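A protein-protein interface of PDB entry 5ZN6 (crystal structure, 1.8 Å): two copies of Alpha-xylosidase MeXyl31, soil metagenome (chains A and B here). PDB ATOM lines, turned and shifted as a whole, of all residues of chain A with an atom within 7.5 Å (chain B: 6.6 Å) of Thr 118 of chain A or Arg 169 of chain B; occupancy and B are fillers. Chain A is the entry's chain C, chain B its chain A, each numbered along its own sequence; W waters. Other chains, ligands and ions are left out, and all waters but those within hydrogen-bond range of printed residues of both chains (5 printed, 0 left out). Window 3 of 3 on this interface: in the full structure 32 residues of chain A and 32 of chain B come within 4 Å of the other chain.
O of Ala 167 of chain B sits at hydrogen-bond distance from NE2 of Gln 172 of chain B. O of Ser 171 of chain B is in hydrogen-bond range of NE2 of Gln 151 of chain B. O of Pro 116 of chain A sits at hydrogen-bond distance from OG1 of Thr 118 of chain A (3.1 Å). The side-chain amide nitrogen of Asn 170 of chain B sits close to the guanidinium group of Arg 441 of chain B, at 3.4 Å. The side-chain amide nitrogen (ND2) of Asn 170 of chain B lies within hydrogen-bond range of the side-chain carboxylate (OE2) of Glu 393 of chain B, at 3.0 Å. The backbone carbonyl oxygen (O) of Gln 172 of chain B is in hydrogen-bond range of the side-chain sulfur (SG) of Cys 442 of chain B (3.6 Å).
Of the 18 printed residues of chain B, 6 touch a printed residue of chain A. Hydrophobic or aromatic side chains of chain B within 4 Å of the printed part of chain A: Tyr 397. Of the 15 printed residues of chain A, 5 touch a printed residue of chain B. Among the printed residues, Asp or Glu carboxylates within 4 Å of a Lys or Arg side-chain nitrogen of the other chain: Arg 100 of chain A with Glu 393 of chain B.
No position is printed for both chains.
Arg 100 of chain A touches Asn 170 of chain B. Pro 116 of chain A touches Asn 170 of chain B (CB to ND2, 3.6 Å). Pro 116 of chain A touches Tyr 397 of chain B. Leu 117 of chain A touches Asn 170 of chain B. CD2 of Leu 117 of chain A touches OG of Ser 171 of chain B, at 3.7 Å. Gln 172 of chain B touches Leu 117 of chain A (CB to CD2, 3.8 Å). O of Leu 117 of chain A touches CE2 of Tyr 397 of chain B, at 3.6 Å. Arg 169 of chain B touches Thr 118 of chain A. His 119 of chain A touches Arg 169 of chain B (CE1 to CZ, 3.4 Å).
Water W1 lies within hydrogen-bond range of the side-chain carboxylate of Glu 393 of chain B (2.5 Å), the side-chain hydroxyl of Tyr 397 of chain B (2.6 Å) and the backbone carbonyl oxygen of Pro 116 of chain A (2.7 Å). Water W5 lies within hydrogen-bond range of OE1 of Gln 172 of chain B (2.7 Å), NE2 of His 119 of chain A (2.7 Å) and OE1 of Glu 165 of chain B (2.8 Å). Water W4 bridges the backbone carbonyl oxygen (O) of Thr 118 of chain A and the guanidinium group (NH1) of Arg 169 of chain B. Water W3 lies within hydrogen-bond range of the side-chain hydroxyl (OG1) of Thr 118 of chain A and the backbone carbonyl oxygen (O) of Ser 395 of chain B. Water W2 lies within hydrogen-bond range of OG of Ser 171 of chain B (2.8 Å) and OG of Ser 115 of chain A (2.9 Å).
Thr 118 of chain A touches one residue of chain B. Of chain A, only Leu 117, Thr 118 and His 119 come within 4 Å of Arg 169 of chain B. Of the printed residues of chain A, Gln 172 of chain B touches Leu 117 (3.8 Å). Of the printed residues of chain B, Leu 117 of chain A touches Arg 169 (3.0 Å), Asn 170 (3.5 Å), Ser 171 (3.7 Å), Gln 172 (3.8 Å) and Tyr 397 (3.6 Å). Ser 395 of chain B touches none of the printed residues of chain A. Gln 168 of chain B touches none of the printed residues of chain A. The nearest residue of chain B that does not touch Thr 118 of chain A is Tyr 397 of chain B (4.4 Å). The nearest printed residue of chain A that does not touch Glu 393 of chain B is Pro 116 of chain A (4.3 Å).
O of Leu 117 of chain A lies within hydrogen-bond range of NH1 of Arg 169 of chain B (3.0 Å). The side-chain carboxylate (OE2) of Glu 393 of chain B lies within salt-bridge range of the guanidinium group (NH2) of Arg 100 of chain A, 3.1 Å away.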
ATOM      1  N   TYR A  96     -27.612 -14.967  -0.205  1.00  0.00           N
ATOM      2  CA  TYR A  96     -26.282 -15.454   0.057  1.00  0.00           C
ATOM      3  C   TYR A  96     -25.525 -15.523  -1.271  1.00  0.00           C
ATOM      4  O   TYR A  96     -25.946 -16.192  -2.218  1.00  0.00           O
ATOM      5  CB  TYR A  96     -26.372 -16.782   0.796  1.00  0.00           C
ATOM      6  CG  TYR A  96     -25.133 -17.639   0.927  1.00  0.00           C
ATOM      7  CD1 TYR A  96     -24.714 -18.423  -0.127  1.00  0.00           C
ATOM      8  CD2 TYR A  96     -24.450 -17.762   2.145  1.00  0.00           C
ATOM      9  CE1 TYR A  96     -23.623 -19.274  -0.015  1.00  0.00           C
ATOM     10  CE2 TYR A  96     -23.344 -18.605   2.260  1.00  0.00           C
ATOM     11  CZ  TYR A  96     -22.949 -19.362   1.168  1.00  0.00           C
ATOM     12  OH  TYR A  96     -21.885 -20.239   1.204  1.00  0.00           O
ATOM     13  N   TRP A  97     -24.438 -14.758  -1.325  1.00  0.00           N
ATOM     14  CA  TRP A  97     -23.528 -14.699  -2.447  1.00  0.00           C
ATOM     15  C   TRP A  97     -22.114 -14.929  -1.903  1.00  0.00           C
ATOM     16  O   TRP A  97     -21.760 -14.369  -0.870  1.00  0.00           O
ATOM     17  CB  TRP A  97     -23.612 -13.314  -3.119  1.00  0.00           C
ATOM     18  CG  TRP A  97     -24.876 -13.070  -3.852  1.00  0.00           C
ATOM     19  CD1 TRP A  97     -26.019 -12.510  -3.347  1.00  0.00           C
ATOM     20  CD2 TRP A  97     -25.152 -13.383  -5.227  1.00  0.00           C
ATOM     21  NE1 TRP A  97     -26.982 -12.453  -4.326  1.00  0.00           N
ATOM     22  CE2 TRP A  97     -26.477 -12.974  -5.488  1.00  0.00           C
ATOM     23  CE3 TRP A  97     -24.405 -13.951  -6.269  1.00  0.00           C
ATOM     24  CZ2 TRP A  97     -27.086 -13.147  -6.737  1.00  0.00           C
ATOM     25  CZ3 TRP A  97     -25.001 -14.115  -7.520  1.00  0.00           C
ATOM     26  CH2 TRP A  97     -26.342 -13.709  -7.741  1.00  0.00           C
ATOM     27  N   ARG A  98     -21.332 -15.766  -2.583  1.00  0.00           N
ATOM     28  CA  ARG A  98     -19.904 -15.951  -2.288  1.00  0.00           C
ATOM     29  C   ARG A  98     -19.141 -16.044  -3.614  1.00  0.00           C
ATOM     30  O   ARG A  98     -18.952 -17.139  -4.152  1.00  0.00           O
ATOM     31  CB  ARG A  98     -19.683 -17.230  -1.450  1.00  0.00           C
ATOM     32  CG  ARG A  98     -20.329 -17.214  -0.077  1.00  0.00           C
ATOM     33  CD  ARG A  98     -19.644 -16.264   0.884  1.00  0.00           C
ATOM     34  NE  ARG A  98     -20.201 -16.370   2.228  1.00  0.00           N
ATOM     35  CZ  ARG A  98     -21.333 -15.796   2.643  1.00  0.00           C
ATOM     36  NH1 ARG A  98     -22.089 -15.070   1.827  1.00  0.00           N
ATOM     37  NH2 ARG A  98     -21.737 -15.983   3.887  1.00  0.00           N
ATOM     38  N   THR A  99     -18.750 -14.897  -4.167  1.00  0.00           N
ATOM     39  CA  THR A  99     -18.045 -14.835  -5.462  1.00  0.00           C
ATOM     40  C   THR A  99     -16.987 -13.718  -5.440  1.00  0.00           C
ATOM     41  O   THR A  99     -16.981 -12.875  -4.531  1.00  0.00           O
ATOM     42  CB  THR A  99     -18.980 -14.518  -6.645  1.00  0.00           C
ATOM     43  OG1 THR A  99     -19.235 -13.112  -6.668  1.00  0.00           O
ATOM     44  CG2 THR A  99     -20.298 -15.263  -6.568  1.00  0.00           C
ATOM     45  N   ARG A 100     -16.087 -13.741  -6.424  1.00  0.00           N
ATOM     46  CA  ARG A 100     -15.163 -12.628  -6.671  1.00  0.00           C
ATOM     47  C   ARG A 100     -15.622 -11.729  -7.818  1.00  0.00           C
ATOM     48  O   ARG A 100     -15.114 -10.614  -7.975  1.00  0.00           O
ATOM     49  CB  ARG A 100     -13.760 -13.158  -6.918  1.00  0.00           C
ATOM     50  CG  ARG A 100     -13.246 -13.888  -5.704  1.00  0.00           C
ATOM     51  CD  ARG A 100     -11.741 -14.086  -5.713  1.00  0.00           C
ATOM     52  NE  ARG A 100     -11.340 -15.068  -6.689  1.00  0.00           N
ATOM     53  CZ  ARG A 100     -10.163 -15.701  -6.708  1.00  0.00           C
ATOM     54  NH1 ARG A 100      -9.217 -15.474  -5.791  1.00  0.00           N
ATOM     55  NH2 ARG A 100      -9.938 -16.588  -7.669  1.00  0.00           N
ATOM     56  N   PHE A 101     -16.606 -12.199  -8.579  1.00  0.00           N
ATOM     57  CA  PHE A 101     -17.035 -11.553  -9.812  1.00  0.00           C
ATOM     58  C   PHE A 101     -18.493 -11.954 -10.035  1.00  0.00           C
ATOM     59  O   PHE A 101     -18.834 -13.142  -9.995  1.00  0.00           O
ATOM     60  CB  PHE A 101     -16.132 -12.024 -10.968  1.00  0.00           C
ATOM     61  CG  PHE A 101     -16.214 -11.178 -12.210  1.00  0.00           C
ATOM     62  CD1 PHE A 101     -15.443 -10.021 -12.335  1.00  0.00           C
ATOM     63  CD2 PHE A 101     -17.022 -11.562 -13.281  1.00  0.00           C
ATOM     64  CE1 PHE A 101     -15.496  -9.247 -13.492  1.00  0.00           C
ATOM     65  CE2 PHE A 101     -17.074 -10.795 -14.450  1.00  0.00           C
ATOM     66  CZ  PHE A 101     -16.310  -9.638 -14.551  1.00  0.00           C
ATOM     67  N   TYR A 113     -19.825 -11.155   1.042  1.00  0.00           N
ATOM     68  CA  TYR A 113     -20.036 -11.705  -0.288  1.00  0.00           C
ATOM     69  C   TYR A 113     -18.754 -12.024  -1.085  1.00  0.00           C
ATOM     70  O   TYR A 113     -18.824 -12.762  -2.067  1.00  0.00           O
ATOM     71  CB  TYR A 113     -20.920 -10.767  -1.120  1.00  0.00           C
ATOM     72  CG  TYR A 113     -22.406 -10.682  -0.758  1.00  0.00           C
ATOM     73  CD1 TYR A 113     -23.025 -11.565   0.159  1.00  0.00           C
ATOM     74  CD2 TYR A 113     -23.218  -9.753  -1.413  1.00  0.00           C
ATOM     75  CE1 TYR A 113     -24.385 -11.478   0.420  1.00  0.00           C
ATOM     76  CE2 TYR A 113     -24.572  -9.676  -1.162  1.00  0.00           C
ATOM     77  CZ  TYR A 113     -25.146 -10.535  -0.250  1.00  0.00           C
ATOM     78  OH  TYR A 113     -26.481 -10.437  -0.028  1.00  0.00           O
ATOM     79  N   SER A 115     -15.677 -13.898  -2.011  1.00  0.00           N
ATOM     80  CA  SER A 115     -15.173 -15.249  -1.798  1.00  0.00           C
ATOM     81  C   SER A 115     -14.813 -15.925  -3.118  1.00  0.00           C
ATOM     82  O   SER A 115     -15.584 -15.860  -4.076  1.00  0.00           O
ATOM     83  CB  SER A 115     -16.237 -16.089  -1.079  1.00  0.00           C
ATOM     84  OG  SER A 115     -15.891 -17.465  -1.050  1.00  0.00           O
ATOM     85  N   PRO A 116     -13.670 -16.631  -3.160  1.00  0.00           N
ATOM     86  CA  PRO A 116     -13.407 -17.464  -4.337  1.00  0.00           C
ATOM     87  C   PRO A 116     -14.257 -18.734  -4.466  1.00  0.00           C
ATOM     88  O   PRO A 116     -14.135 -19.431  -5.483  1.00  0.00           O
ATOM     89  CB  PRO A 116     -11.921 -17.833  -4.199  1.00  0.00           C
ATOM     90  CG  PRO A 116     -11.517 -17.494  -2.814  1.00  0.00           C
ATOM     91  CD  PRO A 116     -12.638 -16.780  -2.119  1.00  0.00           C
ATOM     92  N   LEU A 117     -15.111 -19.043  -3.485  1.00  0.00           N
ATOM     93  CA  LEU A 117     -15.919 -20.270  -3.536  1.00  0.00           C
ATOM     94  C   LEU A 117     -16.827 -20.334  -4.772  1.00  0.00           C
ATOM     95  O   LEU A 117     -16.964 -21.393  -5.372  1.00  0.00           O
ATOM     96  CB  LEU A 117     -16.736 -20.442  -2.252  1.00  0.00           C
ATOM     97  CG  LEU A 117     -15.939 -20.604  -0.950  1.00  0.00           C
ATOM     98  CD1 LEU A 117     -16.865 -20.511   0.251  1.00  0.00           C
ATOM     99  CD2 LEU A 117     -15.114 -21.889  -0.909  1.00  0.00           C
ATOM    100  N   THR A 118     -17.419 -19.195  -5.143  1.00  0.00           N
ATOM    101  CA  THR A 118     -18.292 -19.069  -6.331  1.00  0.00           C
ATOM    102  C   THR A 118     -19.629 -19.796  -6.155  1.00  0.00           C
ATOM    103  O   THR A 118     -19.948 -20.742  -6.880  1.00  0.00           O
ATOM    104  CB  THR A 118     -17.595 -19.467  -7.657  1.00  0.00           C
ATOM    105  OG1 THR A 118     -16.264 -18.944  -7.671  1.00  0.00           O
ATOM    106  CG2 THR A 118     -18.378 -18.916  -8.869  1.00  0.00           C
ATOM    107  N   HIS A 119     -20.403 -19.318  -5.182  1.00  0.00           N
ATOM    108  CA  HIS A 119     -21.779 -19.738  -4.959  1.00  0.00           C
ATOM    109  C   HIS A 119     -22.681 -18.544  -5.236  1.00  0.00           C
ATOM    110  O   HIS A 119     -22.460 -17.469  -4.691  1.00  0.00           O
ATOM    111  CB  HIS A 119     -22.004 -20.193  -3.520  1.00  0.00           C
ATOM    112  CG  HIS A 119     -21.230 -21.412  -3.128  1.00  0.00           C
ATOM    113  ND1 HIS A 119     -21.229 -22.571  -3.875  1.00  0.00           N
ATOM    114  CD2 HIS A 119     -20.482 -21.672  -2.028  1.00  0.00           C
ATOM    115  CE1 HIS A 119     -20.494 -23.485  -3.262  1.00  0.00           C
ATOM    116  NE2 HIS A 119     -20.016 -22.958  -2.148  1.00  0.00           N
ATOM    117  N   GLU A 120     -23.684 -18.745  -6.085  1.00  0.00           N
ATOM    118  CA  GLU A 120     -24.670 -17.713  -6.409  1.00  0.00           C
ATOM    119  C   GLU A 120     -25.942 -17.855  -5.583  1.00  0.00           C
ATOM    120  O   GLU A 120     -26.306 -18.955  -5.216  1.00  0.00           O
ATOM    121  CB  GLU A 120     -25.096 -17.856  -7.858  1.00  0.00           C
ATOM    122  CG  GLU A 120     -24.011 -17.704  -8.894  1.00  0.00           C
ATOM    123  CD  GLU A 120     -24.631 -17.885 -10.262  1.00  0.00           C
ATOM    124  OE1 GLU A 120     -25.054 -19.033 -10.588  1.00  0.00           O
ATOM    125  OE2 GLU A 120     -24.766 -16.867 -10.966  1.00  0.00           O
ATOM    126  N   GLU A 123     -29.125 -19.746  -8.381  1.00  0.00           N
ATOM    127  CA  GLU A 123     -28.388 -20.650  -9.235  1.00  0.00           C
ATOM    128  C   GLU A 123     -29.373 -21.454 -10.067  1.00  0.00           C
ATOM    129  O   GLU A 123     -30.020 -22.357  -9.545  1.00  0.00           O
ATOM    130  CB  GLU A 123     -27.535 -21.589  -8.380  1.00  0.00           C
ATOM    131  CG  GLU A 123     -26.606 -22.487  -9.185  1.00  0.00           C
ATOM    132  CD  GLU A 123     -26.055 -23.669  -8.394  1.00  0.00           C
ATOM    133  OE1 GLU A 123     -26.117 -23.678  -7.162  1.00  0.00           O
ATOM    134  OE2 GLU A 123     -25.562 -24.620  -9.014  1.00  0.00           O
ATOM    135  N   ARG A 137     -30.270 -19.411  -2.410  1.00  0.00           N
ATOM    136  CA  ARG A 137     -29.525 -19.344  -1.161  1.00  0.00           C
ATOM    137  C   ARG A 137     -29.742 -18.009  -0.466  1.00  0.00           C
ATOM    138  O   ARG A 137     -29.763 -16.969  -1.118  1.00  0.00           O
ATOM    139  CB  ARG A 137     -28.040 -19.533  -1.444  1.00  0.00           C
ATOM    140  CG  ARG A 137     -27.703 -20.835  -2.158  1.00  0.00           C
ATOM    141  CD  ARG A 137     -26.199 -20.987  -2.271  1.00  0.00           C
ATOM    142  NE  ARG A 137     -25.821 -22.273  -2.836  1.00  0.00           N
ATOM    143  CZ  ARG A 137     -25.705 -22.567  -4.136  1.00  0.00           C
ATOM    144  NH1 ARG A 137     -25.938 -21.670  -5.094  1.00  0.00           N
ATOM    145  NH2 ARG A 137     -25.364 -23.799  -4.482  1.00  0.00           N
ATOM    146  N   GLN B 151     -11.606 -27.429   6.562  1.00  0.00           N
ATOM    147  CA  GLN B 151     -11.516 -25.978   6.573  1.00  0.00           C
ATOM    148  C   GLN B 151     -12.689 -25.370   5.816  1.00  0.00           C
ATOM    149  O   GLN B 151     -12.709 -25.424   4.584  1.00  0.00           O
ATOM    150  CB  GLN B 151     -10.216 -25.591   5.893  1.00  0.00           C
ATOM    151  CG  GLN B 151      -9.852 -24.125   5.921  1.00  0.00           C
ATOM    152  CD  GLN B 151      -8.678 -23.898   5.004  1.00  0.00           C
ATOM    153  OE1 GLN B 151      -7.509 -24.107   5.398  1.00  0.00           O
ATOM    154  NE2 GLN B 151      -8.975 -23.548   3.752  1.00  0.00           N
ATOM    155  N   GLU B 165     -20.081 -28.881   2.230  1.00  0.00           N
ATOM    156  CA  GLU B 165     -19.832 -29.485   0.932  1.00  0.00           C
ATOM    157  C   GLU B 165     -18.574 -30.337   0.992  1.00  0.00           C
ATOM    158  O   GLU B 165     -17.523 -29.872   1.447  1.00  0.00           O
ATOM    159  CB  GLU B 165     -19.670 -28.408  -0.119  1.00  0.00           C
ATOM    160  CG  GLU B 165     -19.522 -28.943  -1.531  1.00  0.00           C
ATOM    161  CD  GLU B 165     -19.135 -27.869  -2.526  1.00  0.00           C
ATOM    162  OE1 GLU B 165     -18.386 -26.918  -2.176  1.00  0.00           O
ATOM    163  OE2 GLU B 165     -19.563 -27.992  -3.690  1.00  0.00           O
ATOM    164  N   ALA B 167     -16.182 -31.087  -1.127  1.00  0.00           N
ATOM    165  CA  ALA B 167     -15.501 -30.698  -2.355  1.00  0.00           C
ATOM    166  C   ALA B 167     -14.399 -29.718  -2.023  1.00  0.00           C
ATOM    167  O   ALA B 167     -14.450 -29.084  -0.975  1.00  0.00           O
ATOM    168  CB  ALA B 167     -16.470 -30.052  -3.319  1.00  0.00           C
ATOM    169  N   GLN B 168     -13.443 -29.591  -2.943  1.00  0.00           N
ATOM    170  CA  GLN B 168     -12.296 -28.706  -2.805  1.00  0.00           C
ATOM    171  C   GLN B 168     -12.495 -27.483  -3.678  1.00  0.00           C
ATOM    172  O   GLN B 168     -12.615 -27.606  -4.889  1.00  0.00           O
ATOM    173  CB  GLN B 168     -11.016 -29.424  -3.222  1.00  0.00           C
ATOM    174  CG  GLN B 168     -10.846 -30.838  -2.663  1.00  0.00           C
ATOM    175  CD  GLN B 168     -10.736 -30.922  -1.141  1.00  0.00           C
ATOM    176  OE1 GLN B 168     -11.075 -29.988  -0.413  1.00  0.00           O
ATOM    177  NE2 GLN B 168     -10.234 -32.063  -0.654  1.00  0.00           N
ATOM    178  N   ARG B 169     -12.508 -26.315  -3.043  1.00  0.00           N
ATOM    179  CA  ARG B 169     -12.561 -25.021  -3.705  1.00  0.00           C
ATOM    180  C   ARG B 169     -11.559 -24.103  -3.007  1.00  0.00           C
ATOM    181  O   ARG B 169     -11.216 -24.328  -1.843  1.00  0.00           O
ATOM    182  CB  ARG B 169     -13.948 -24.398  -3.559  1.00  0.00           C
ATOM    183  CG  ARG B 169     -15.113 -25.208  -4.072  1.00  0.00           C
ATOM    184  CD  ARG B 169     -16.423 -24.518  -3.708  1.00  0.00           C
ATOM    185  NE  ARG B 169     -17.567 -25.283  -4.188  1.00  0.00           N
ATOM    186  CZ  ARG B 169     -18.269 -25.058  -5.310  1.00  0.00           C
ATOM    187  NH1 ARG B 169     -18.030 -24.036  -6.140  1.00  0.00           N
ATOM    188  NH2 ARG B 169     -19.263 -25.881  -5.602  1.00  0.00           N
ATOM    189  N   ASN B 170     -11.090 -23.075  -3.713  1.00  0.00           N
ATOM    190  CA  ASN B 170     -10.154 -22.063  -3.134  1.00  0.00           C
ATOM    191  C   ASN B 170     -10.738 -21.499  -1.820  1.00  0.00           C
ATOM    192  O   ASN B 170     -11.831 -20.934  -1.822  1.00  0.00           O
ATOM    193  CB  ASN B 170      -9.905 -20.958  -4.181  1.00  0.00           C
ATOM    194  CG  ASN B 170      -8.892 -19.884  -3.734  1.00  0.00           C
ATOM    195  OD1 ASN B 170      -8.411 -19.842  -2.585  1.00  0.00           O
ATOM    196  ND2 ASN B 170      -8.582 -18.984  -4.665  1.00  0.00           N
ATOM    197  N   SER B 171      -9.999 -21.708  -0.718  1.00  0.00           N
ATOM    198  CA  SER B 171     -10.355 -21.348   0.671  1.00  0.00           C
ATOM    199  C   SER B 171     -11.169 -22.394   1.461  1.00  0.00           C
ATOM    200  O   SER B 171     -11.463 -22.177   2.625  1.00  0.00           O
ATOM    201  CB  SER B 171     -10.976 -19.933   0.822  1.00  0.00           C
ATOM    202  OG  SER B 171     -12.356 -19.879   0.481  1.00  0.00           O
ATOM    203  N   GLN B 172     -11.469 -23.537   0.833  1.00  0.00           N
ATOM    204  CA  GLN B 172     -12.141 -24.655   1.475  1.00  0.00           C
ATOM    205  C   GLN B 172     -11.320 -25.929   1.282  1.00  0.00           C
ATOM    206  O   GLN B 172     -10.747 -26.152   0.209  1.00  0.00           O
ATOM    207  CB  GLN B 172     -13.533 -24.804   0.873  1.00  0.00           C
ATOM    208  CG  GLN B 172     -14.386 -25.954   1.372  1.00  0.00           C
ATOM    209  CD  GLN B 172     -15.750 -25.904   0.720  1.00  0.00           C
ATOM    210  OE1 GLN B 172     -16.529 -24.982   0.972  1.00  0.00           O
ATOM    211  NE2 GLN B 172     -16.010 -26.844  -0.187  1.00  0.00           N
ATOM    212  N   ALA B 173     -11.262 -26.747   2.331  1.00  0.00           N
ATOM    213  CA  ALA B 173     -10.599 -28.038   2.297  1.00  0.00           C
ATOM    214  C   ALA B 173     -11.505 -29.041   2.988  1.00  0.00           C
ATOM    215  O   ALA B 173     -11.822 -28.876   4.178  1.00  0.00           O
ATOM    216  CB  ALA B 173      -9.240 -27.984   2.999  1.00  0.00           C
ATOM    217  N   SER B 174     -11.953 -30.045   2.238  1.00  0.00           N
ATOM    218  CA  SER B 174     -12.688 -31.172   2.797  1.00  0.00           C
ATOM    219  C   SER B 174     -11.691 -32.205   3.307  1.00  0.00           C
ATOM    220  O   SER B 174     -10.950 -32.818   2.521  1.00  0.00           O
ATOM    221  CB  SER B 174     -13.612 -31.787   1.759  1.00  0.00           C
ATOM    222  OG  SER B 174     -14.339 -32.858   2.328  1.00  0.00           O
ATOM    223  N   GLU B 391      -6.545 -27.472  -5.197  1.00  0.00           N
ATOM    224  CA  GLU B 391      -7.862 -28.073  -5.139  1.00  0.00           C
ATOM    225  C   GLU B 391      -8.152 -29.148  -6.224  1.00  0.00           C
ATOM    226  O   GLU B 391      -8.648 -30.216  -5.843  1.00  0.00           O
ATOM    227  CB  GLU B 391      -8.951 -26.991  -5.129  1.00  0.00           C
ATOM    228  CG  GLU B 391      -8.854 -26.041  -3.937  1.00  0.00           C
ATOM    229  CD  GLU B 391      -7.800 -24.937  -4.093  1.00  0.00           C
ATOM    230  OE1 GLU B 391      -7.372 -24.661  -5.230  1.00  0.00           O
ATOM    231  OE2 GLU B 391      -7.391 -24.346  -3.066  1.00  0.00           O
ATOM    232  N   PRO B 392      -7.884 -28.925  -7.531  1.00  0.00           N
ATOM    233  CA  PRO B 392      -7.333 -27.700  -8.129  1.00  0.00           C
ATOM    234  C   PRO B 392      -8.389 -26.647  -8.446  1.00  0.00           C
ATOM    235  O   PRO B 392      -9.582 -26.972  -8.484  1.00  0.00           O
ATOM    236  CB  PRO B 392      -6.714 -28.219  -9.427  1.00  0.00           C
ATOM    237  CG  PRO B 392      -7.655 -29.322  -9.852  1.00  0.00           C
ATOM    238  CD  PRO B 392      -8.264 -29.893  -8.580  1.00  0.00           C
ATOM    239  N   GLU B 393      -7.954 -25.396  -8.637  1.00  0.00           N
ATOM    240  CA  GLU B 393      -8.874 -24.269  -8.872  1.00  0.00           C
ATOM    241  C   GLU B 393      -9.341 -24.186 -10.328  1.00  0.00           C
ATOM    242  O   GLU B 393      -8.906 -23.316 -11.103  1.00  0.00           O
ATOM    243  CB  GLU B 393      -8.272 -22.922  -8.435  1.00  0.00           C
ATOM    244  CG  GLU B 393      -9.279 -21.760  -8.478  1.00  0.00           C
ATOM    245  CD  GLU B 393      -8.785 -20.481  -7.819  1.00  0.00           C
ATOM    246  OE1 GLU B 393      -7.560 -20.250  -7.754  1.00  0.00           O
ATOM    247  OE2 GLU B 393      -9.631 -19.691  -7.356  1.00  0.00           O
ATOM    248  N   SER B 395     -11.537 -23.012 -13.293  1.00  0.00           N
ATOM    249  CA  SER B 395     -12.168 -21.727 -13.562  1.00  0.00           C
ATOM    250  C   SER B 395     -13.670 -21.794 -13.301  1.00  0.00           C
ATOM    251  O   SER B 395     -14.286 -20.780 -12.916  1.00  0.00           O
ATOM    252  CB  SER B 395     -11.904 -21.261 -14.996  1.00  0.00           C
ATOM    253  OG  SER B 395     -10.572 -20.797 -15.126  1.00  0.00           O
ATOM    254  N   TYR B 397     -16.247 -24.651 -11.273  1.00  0.00           N
ATOM    255  CA  TYR B 397     -16.250 -25.864 -10.444  1.00  0.00           C
ATOM    256  C   TYR B 397     -17.376 -26.832 -10.860  1.00  0.00           C
ATOM    257  O   TYR B 397     -18.244 -27.191 -10.069  1.00  0.00           O
ATOM    258  CB  TYR B 397     -16.353 -25.519  -8.950  1.00  0.00           C
ATOM    259  CG  TYR B 397     -15.176 -24.792  -8.327  1.00  0.00           C
ATOM    260  CD1 TYR B 397     -13.967 -25.455  -8.066  1.00  0.00           C
ATOM    261  CD2 TYR B 397     -15.287 -23.451  -7.924  1.00  0.00           C
ATOM    262  CE1 TYR B 397     -12.908 -24.799  -7.451  1.00  0.00           C
ATOM    263  CE2 TYR B 397     -14.234 -22.785  -7.327  1.00  0.00           C
ATOM    264  CZ  TYR B 397     -13.049 -23.453  -7.093  1.00  0.00           C
ATOM    265  OH  TYR B 397     -12.009 -22.780  -6.497  1.00  0.00           O
ATOM    266  N   PHE B 399     -17.746 -30.148 -11.328  1.00  0.00           N
ATOM    267  CA  PHE B 399     -17.007 -31.372 -10.979  1.00  0.00           C
ATOM    268  C   PHE B 399     -17.318 -32.533 -11.915  1.00  0.00           C
ATOM    269  O   PHE B 399     -16.449 -33.325 -12.255  1.00  0.00           O
ATOM    270  CB  PHE B 399     -17.298 -31.767  -9.531  1.00  0.00           C
ATOM    271  CG  PHE B 399     -16.949 -30.696  -8.544  1.00  0.00           C
ATOM    272  CD1 PHE B 399     -15.631 -30.288  -8.388  1.00  0.00           C
ATOM    273  CD2 PHE B 399     -17.944 -30.058  -7.803  1.00  0.00           C
ATOM    274  CE1 PHE B 399     -15.305 -29.282  -7.490  1.00  0.00           C
ATOM    275  CE2 PHE B 399     -17.622 -29.050  -6.911  1.00  0.00           C
ATOM    276  CZ  PHE B 399     -16.300 -28.669  -6.750  1.00  0.00           C
ATOM    277  N   ARG B 441      -2.400 -25.396  -0.457  1.00  0.00           N
ATOM    278  CA  ARG B 441      -3.647 -24.646  -0.305  1.00  0.00           C
ATOM    279  C   ARG B 441      -4.844 -25.501   0.106  1.00  0.00           C
ATOM    280  O   ARG B 441      -5.882 -24.960   0.500  1.00  0.00           O
ATOM    281  CB  ARG B 441      -4.004 -23.837  -1.544  1.00  0.00           C
ATOM    282  CG  ARG B 441      -4.876 -22.644  -1.152  1.00  0.00           C
ATOM    283  CD  ARG B 441      -4.936 -21.603  -2.226  1.00  0.00           C
ATOM    284  NE  ARG B 441      -5.714 -22.070  -3.352  1.00  0.00           N
ATOM    285  CZ  ARG B 441      -5.932 -21.352  -4.443  1.00  0.00           C
ATOM    286  NH1 ARG B 441      -5.424 -20.117  -4.550  1.00  0.00           N
ATOM    287  NH2 ARG B 441      -6.685 -21.848  -5.416  1.00  0.00           N
ATOM    288  N   CYS B 442      -4.707 -26.819   0.008  1.00  0.00           N
ATOM    289  CA  CYS B 442      -5.821 -27.729   0.239  1.00  0.00           C
ATOM    290  C   CYS B 442      -5.270 -29.088   0.687  1.00  0.00           C
ATOM    291  O   CYS B 442      -4.052 -29.320   0.670  1.00  0.00           O
ATOM    292  CB  CYS B 442      -6.662 -27.838  -1.020  1.00  0.00           C
ATOM    293  SG  CYS B 442      -8.294 -28.568  -0.775  1.00  0.00           S
HETATM  294  O   HOH W   1     -12.118 -20.221  -7.170  1.00  0.00           O
HETATM  295  O   HOH W   2     -13.912 -17.590   1.048  1.00  0.00           O
HETATM  296  O   HOH W   3     -15.370 -20.041 -10.038  1.00  0.00           O
HETATM  297  O   HOH W   4     -19.122 -22.794  -8.504  1.00  0.00           O
HETATM  298  O   HOH W   5     -18.762 -24.710  -0.457  1.00  0.00           O
